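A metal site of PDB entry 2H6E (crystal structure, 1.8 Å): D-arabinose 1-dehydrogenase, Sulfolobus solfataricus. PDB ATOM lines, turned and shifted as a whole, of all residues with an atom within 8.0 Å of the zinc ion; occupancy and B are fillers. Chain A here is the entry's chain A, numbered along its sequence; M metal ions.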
ATOM      1  N   GLY A  39       4.940  14.003  -2.001  1.00  0.00           N
ATOM      2  CA  GLY A  39       4.896  15.358  -2.567  1.00  0.00           C
ATOM      3  C   GLY A  39       3.492  15.860  -2.858  1.00  0.00           C
ATOM      4  O   GLY A  39       2.576  15.063  -3.048  1.00  0.00           O
ATOM      5  N   VAL A  40       3.328  17.186  -2.868  1.00  0.00           N
ATOM      6  CA  VAL A  40       2.034  17.848  -3.115  1.00  0.00           C
ATOM      7  C   VAL A  40       2.033  18.535  -4.501  1.00  0.00           C
ATOM      8  O   VAL A  40       2.824  19.441  -4.766  1.00  0.00           O
ATOM      9  CB  VAL A  40       1.722  18.867  -1.992  1.00  0.00           C
ATOM     10  CG1 VAL A  40       0.378  19.550  -2.242  1.00  0.00           C
ATOM     11  CG2 VAL A  40       1.728  18.171  -0.626  1.00  0.00           C
ATOM     12  N   CYS A  41       1.149  18.083  -5.388  1.00  0.00           N
ATOM     13  CA  CYS A  41       1.124  18.521  -6.787  1.00  0.00           C
ATOM     14  C   CYS A  41      -0.059  19.427  -7.097  1.00  0.00           C
ATOM     15  O   CYS A  41      -1.068  19.397  -6.407  1.00  0.00           O
ATOM     16  CB  CYS A  41       1.011  17.320  -7.706  1.00  0.00           C
ATOM     17  SG  CYS A  41       1.354  17.655  -9.462  1.00  0.00           S
ATOM     18  N   ARG A  42       0.089  20.243  -8.147  1.00  0.00           N
ATOM     19  CA  ARG A  42      -1.058  20.949  -8.734  1.00  0.00           C
ATOM     20  C   ARG A  42      -2.146  19.968  -9.178  1.00  0.00           C
ATOM     21  O   ARG A  42      -3.323  20.331  -9.202  1.00  0.00           O
ATOM     22  CB  ARG A  42      -0.626  21.835  -9.921  1.00  0.00           C
ATOM     23  CG  ARG A  42       0.095  23.122  -9.511  1.00  0.00           C
ATOM     24  CD  ARG A  42      -0.215  24.285 -10.434  1.00  0.00           C
ATOM     25  N   THR A  43      -1.762  18.751  -9.546  1.00  0.00           N
ATOM     26  CA  THR A  43      -2.730  17.699  -9.861  1.00  0.00           C
ATOM     27  C   THR A  43      -3.608  17.322  -8.654  1.00  0.00           C
ATOM     28  O   THR A  43      -4.807  17.081  -8.823  1.00  0.00           O
ATOM     29  CB  THR A  43      -2.063  16.460 -10.459  1.00  0.00           C
ATOM     30  OG1 THR A  43      -1.543  16.788 -11.749  1.00  0.00           O
ATOM     31  CG2 THR A  43      -3.068  15.314 -10.595  1.00  0.00           C
ATOM     32  N   ASP A  44      -3.030  17.292  -7.449  1.00  0.00           N
ATOM     33  CA  ASP A  44      -3.807  17.008  -6.229  1.00  0.00           C
ATOM     34  C   ASP A  44      -4.881  18.051  -6.009  1.00  0.00           C
ATOM     35  O   ASP A  44      -5.972  17.728  -5.530  1.00  0.00           O
ATOM     36  CB  ASP A  44      -2.928  16.969  -4.975  1.00  0.00           C
ATOM     37  CG  ASP A  44      -1.986  15.780  -4.934  1.00  0.00           C
ATOM     38  OD1 ASP A  44      -2.466  14.636  -4.766  1.00  0.00           O
ATOM     39  OD2 ASP A  44      -0.761  15.993  -5.051  1.00  0.00           O
ATOM     40  N   ARG A  46      -6.333  19.848  -8.373  1.00  0.00           N
ATOM     41  CA  ARG A  46      -7.374  19.701  -9.386  1.00  0.00           C
ATOM     42  C   ARG A  46      -8.331  18.562  -9.016  1.00  0.00           C
ATOM     43  O   ARG A  46      -9.530  18.652  -9.265  1.00  0.00           O
ATOM     44  CB  ARG A  46      -6.762  19.463 -10.769  1.00  0.00           C
ATOM     45  CG  ARG A  46      -6.192  20.728 -11.402  1.00  0.00           C
ATOM     46  CD  ARG A  46      -5.970  20.528 -12.904  1.00  0.00           C
ATOM     47  NE  ARG A  46      -4.949  19.517 -13.175  1.00  0.00           N
ATOM     48  CZ  ARG A  46      -3.647  19.754 -13.293  1.00  0.00           C
ATOM     49  NH1 ARG A  46      -3.153  20.987 -13.148  1.00  0.00           N
ATOM     50  NH2 ARG A  46      -2.819  18.757 -13.551  1.00  0.00           N
ATOM     51  N   GLU A  52     -10.820  17.219 -12.011  1.00  0.00           N
ATOM     52  CA  GLU A  52     -10.073  16.170 -12.690  1.00  0.00           C
ATOM     53  C   GLU A  52     -10.302  14.819 -12.000  1.00  0.00           C
ATOM     54  O   GLU A  52     -10.107  14.700 -10.783  1.00  0.00           O
ATOM     55  CB  GLU A  52      -8.567  16.486 -12.725  1.00  0.00           C
ATOM     56  CG  GLU A  52      -7.717  15.352 -13.294  1.00  0.00           C
ATOM     57  CD  GLU A  52      -6.273  15.753 -13.532  1.00  0.00           C
ATOM     58  OE1 GLU A  52      -6.040  16.883 -14.021  1.00  0.00           O
ATOM     59  OE2 GLU A  52      -5.375  14.919 -13.266  1.00  0.00           O
ATOM     60  N   LYS A  54      -9.558  10.731 -13.203  1.00  0.00           N
ATOM     61  CA  LYS A  54      -9.162   9.680 -14.139  1.00  0.00           C
ATOM     62  C   LYS A  54      -9.963   8.403 -13.875  1.00  0.00           C
ATOM     63  O   LYS A  54     -10.645   8.298 -12.850  1.00  0.00           O
ATOM     64  CB  LYS A  54      -7.651   9.432 -14.057  1.00  0.00           C
ATOM     65  CG  LYS A  54      -6.848  10.563 -14.705  1.00  0.00           C
ATOM     66  CD  LYS A  54      -5.360  10.492 -14.429  1.00  0.00           C
ATOM     67  CE  LYS A  54      -4.635  11.726 -14.995  1.00  0.00           C
ATOM     68  NZ  LYS A  54      -3.165  11.649 -14.827  1.00  0.00           N
ATOM     69  N   HIS A  65       0.422  11.225  -5.077  1.00  0.00           N
ATOM     70  CA  HIS A  65       0.906  10.339  -6.127  1.00  0.00           C
ATOM     71  C   HIS A  65       2.421  10.481  -6.346  1.00  0.00           C
ATOM     72  O   HIS A  65       2.967   9.971  -7.328  1.00  0.00           O
ATOM     73  CB  HIS A  65       0.146  10.637  -7.429  1.00  0.00           C
ATOM     74  CG  HIS A  65       0.177  12.082  -7.835  1.00  0.00           C
ATOM     75  ND1 HIS A  65      -0.737  13.008  -7.371  1.00  0.00           N
ATOM     76  CD2 HIS A  65       0.969  12.758  -8.705  1.00  0.00           C
ATOM     77  CE1 HIS A  65      -0.491  14.182  -7.914  1.00  0.00           C
ATOM     78  NE2 HIS A  65       0.533  14.070  -8.731  1.00  0.00           N
ATOM     79  N   GLU A  66       3.099  11.153  -5.401  1.00  0.00           N
ATOM     80  CA  GLU A  66       4.500  11.529  -5.581  1.00  0.00           C
ATOM     81  C   GLU A  66       5.266  10.992  -4.380  1.00  0.00           C
ATOM     82  O   GLU A  66       5.573  11.730  -3.440  1.00  0.00           O
ATOM     83  CB  GLU A  66       4.617  13.057  -5.702  1.00  0.00           C
ATOM     84  CG  GLU A  66       6.009  13.574  -6.097  1.00  0.00           C
ATOM     85  CD  GLU A  66       6.042  15.075  -6.427  1.00  0.00           C
ATOM     86  OE1 GLU A  66       5.934  15.893  -5.483  1.00  0.00           O
ATOM     87  OE2 GLU A  66       6.204  15.448  -7.610  1.00  0.00           O
ATOM     88  N   ALA A  90       4.429   6.048 -10.492  1.00  0.00           N
ATOM     89  CA  ALA A  90       3.049   6.349 -10.145  1.00  0.00           C
ATOM     90  C   ALA A  90       1.980   5.804 -11.079  1.00  0.00           C
ATOM     91  O   ALA A  90       0.805   5.813 -10.713  1.00  0.00           O
ATOM     92  CB  ALA A  90       2.881   7.867 -10.010  1.00  0.00           C
ATOM     93  N   GLN A 116      -4.313   9.106  -7.156  1.00  0.00           N
ATOM     94  CA  GLN A 116      -5.221   9.649  -8.178  1.00  0.00           C
ATOM     95  C   GLN A 116      -6.416   8.713  -8.437  1.00  0.00           C
ATOM     96  O   GLN A 116      -7.541   9.212  -8.640  1.00  0.00           O
ATOM     97  CB  GLN A 116      -4.481   9.980  -9.497  1.00  0.00           C
ATOM     98  CG  GLN A 116      -3.467  11.153  -9.443  1.00  0.00           C
ATOM     99  CD  GLN A 116      -2.810  11.456 -10.807  1.00  0.00           C
ATOM    100  OE1 GLN A 116      -3.482  11.498 -11.849  1.00  0.00           O
ATOM    101  NE2 GLN A 116      -1.497  11.666 -10.807  1.00  0.00           N
ATOM    102  N   PRO A 147       9.679  13.994  -4.781  1.00  0.00           N
ATOM    103  CA  PRO A 147       9.294  14.734  -6.009  1.00  0.00           C
ATOM    104  C   PRO A 147       9.742  14.137  -7.338  1.00  0.00           C
ATOM    105  O   PRO A 147       9.166  14.452  -8.384  1.00  0.00           O
ATOM    106  CB  PRO A 147       9.951  16.104  -5.830  1.00  0.00           C
ATOM    107  CG  PRO A 147      10.185  16.216  -4.362  1.00  0.00           C
ATOM    108  CD  PRO A 147      10.532  14.835  -3.923  1.00  0.00           C
ATOM    109  N   ALA A 149       9.300  11.130  -8.129  1.00  0.00           N
ATOM    110  CA  ALA A 149       8.218  10.231  -8.529  1.00  0.00           C
ATOM    111  C   ALA A 149       7.180  10.903  -9.429  1.00  0.00           C
ATOM    112  O   ALA A 149       6.358  10.225 -10.000  1.00  0.00           O
ATOM    113  CB  ALA A 149       7.526   9.626  -7.324  1.00  0.00           C
ATOM    114  N   ASP A 150       7.189  12.227  -9.519  1.00  0.00           N
ATOM    115  CA  ASP A 150       6.283  12.912 -10.462  1.00  0.00           C
ATOM    116  C   ASP A 150       6.889  14.108 -11.165  1.00  0.00           C
ATOM    117  O   ASP A 150       7.164  14.026 -12.367  1.00  0.00           O
ATOM    118  CB  ASP A 150       4.956  13.200  -9.761  1.00  0.00           C
ATOM    119  CG  ASP A 150       4.098  14.183 -10.488  1.00  0.00           C
ATOM    120  OD1 ASP A 150       4.058  14.192 -11.732  1.00  0.00           O
ATOM    121  OD2 ASP A 150       3.440  14.980  -9.780  1.00  0.00           O
ATOM    122  N   ALA A 151       7.134  15.215 -10.461  1.00  0.00           N
ATOM    123  CA  ALA A 151       7.810  16.381 -11.063  1.00  0.00           C
ATOM    124  C   ALA A 151       9.088  15.996 -11.812  1.00  0.00           C
ATOM    125  O   ALA A 151       9.298  16.436 -12.958  1.00  0.00           O
ATOM    126  CB  ALA A 151       8.123  17.451  -9.992  1.00  0.00           C
ATOM    127  N   THR A 154       8.293  13.450 -14.874  1.00  0.00           N
ATOM    128  CA  THR A 154       7.567  14.197 -15.895  1.00  0.00           C
ATOM    129  C   THR A 154       8.521  15.150 -16.615  1.00  0.00           C
ATOM    130  O   THR A 154       8.478  15.261 -17.844  1.00  0.00           O
ATOM    131  CB  THR A 154       6.369  14.974 -15.291  1.00  0.00           C
ATOM    132  OG1 THR A 154       5.489  14.040 -14.663  1.00  0.00           O
ATOM    133  CG2 THR A 154       5.583  15.741 -16.349  1.00  0.00           C
ATOM    134  N   LEU A 182       7.562  21.711 -11.311  1.00  0.00           N
ATOM    135  CA  LEU A 182       8.093  21.070 -12.519  1.00  0.00           C
ATOM    136  C   LEU A 182       9.352  21.782 -13.025  1.00  0.00           C
ATOM    137  O   LEU A 182      10.298  21.133 -13.462  1.00  0.00           O
ATOM    138  CB  LEU A 182       7.047  21.044 -13.639  1.00  0.00           C
ATOM    139  CG  LEU A 182       5.838  20.122 -13.493  1.00  0.00           C
ATOM    140  CD1 LEU A 182       4.604  20.801 -14.112  1.00  0.00           C
ATOM    141  CD2 LEU A 182       6.096  18.722 -14.123  1.00  0.00           C
ATOM    142  N   ASN A 293       2.926  13.247 -20.890  1.00  0.00           N
ATOM    143  CA  ASN A 293       2.434  12.771 -19.603  1.00  0.00           C
ATOM    144  C   ASN A 293       3.467  11.888 -18.924  1.00  0.00           C
ATOM    145  O   ASN A 293       3.796  10.833 -19.426  1.00  0.00           O
ATOM    146  CB  ASN A 293       1.138  11.984 -19.793  1.00  0.00           C
ATOM    147  CG  ASN A 293       0.518  11.545 -18.460  1.00  0.00           C
ATOM    148  OD1 ASN A 293       0.764  12.150 -17.409  1.00  0.00           O
ATOM    149  ND2 ASN A 293      -0.274  10.506 -18.499  1.00  0.00           N
ATOM    150  N   TYR A 294       3.991  12.360 -17.800  1.00  0.00           N
ATOM    151  CA  TYR A 294       4.883  11.554 -16.951  1.00  0.00           C
ATOM    152  C   TYR A 294       6.085  11.018 -17.748  1.00  0.00           C
ATOM    153  O   TYR A 294       6.604  11.726 -18.609  1.00  0.00           O
ATOM    154  CB  TYR A 294       4.045  10.445 -16.286  1.00  0.00           C
ATOM    155  CG  TYR A 294       4.638   9.822 -15.039  1.00  0.00           C
ATOM    156  CD1 TYR A 294       5.208  10.606 -14.045  1.00  0.00           C
ATOM    157  CD2 TYR A 294       4.582   8.436 -14.828  1.00  0.00           C
ATOM    158  CE1 TYR A 294       5.711  10.045 -12.892  1.00  0.00           C
ATOM    159  CE2 TYR A 294       5.095   7.873 -13.672  1.00  0.00           C
ATOM    160  CZ  TYR A 294       5.656   8.670 -12.712  1.00  0.00           C
ATOM    161  OH  TYR A 294       6.172   8.122 -11.558  1.00  0.00           O
ATOM    162  N   ARG A 339       9.265  22.576  -4.204  1.00  0.00           N
ATOM    163  CA  ARG A 339       8.291  21.503  -4.019  1.00  0.00           C
ATOM    164  C   ARG A 339       8.014  21.251  -2.536  1.00  0.00           C
ATOM    165  O   ARG A 339       8.945  21.094  -1.743  1.00  0.00           O
ATOM    166  CB  ARG A 339       8.825  20.215  -4.644  1.00  0.00           C
ATOM    167  CG  ARG A 339       7.771  19.162  -4.956  1.00  0.00           C
ATOM    168  CD  ARG A 339       6.713  19.725  -5.900  1.00  0.00           C
ATOM    169  NE  ARG A 339       6.138  18.709  -6.762  1.00  0.00           N
ATOM    170  CZ  ARG A 339       5.189  18.938  -7.667  1.00  0.00           C
ATOM    171  NH1 ARG A 339       4.726  17.937  -8.414  1.00  0.00           N
ATOM    172  NH2 ARG A 339       4.700  20.173  -7.849  1.00  0.00           N
HETATM  173 ZN    ZN M   1       1.720  15.449 -10.216  1.00  0.00          ZN
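The side-chain carboxylate of Asp 150 lies close to the guanidinium group of Arg 339, 3.5 Å away. O of Asp 150 is in hydrogen-bond range of OG1 of Thr 154. The side-chain sulfur (SG) of Cys 41 sits close to the backbone NH (N) of Thr 43 (3.3 Å). The side-chain sulfur (SG) of Cys 41 sits close to the guanidinium group (NH1) of Arg 339 (3.5 Å). N of Cys 41 lies within hydrogen-bond range of OD2 of Asp 44 (2.9 Å). The guanidinium group (NH2) of Arg 46 sits at hydrogen-bond distance from the side-chain hydroxyl (OG1) of Thr 43.
Thr 43 touches the zinc ion. The nearest printed residue that does not touch the zinc ion is Arg 339 (4.3 Å).
The zinc ion is bound by the side-chain carboxylate of Asp 150 (1.8 Å), a ring nitrogen (NE2) of His 65 (2.3 Å) and the side-chain sulfur of Cys 41 (2.4 Å). The zinc ion has three donor atoms within binding distance.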
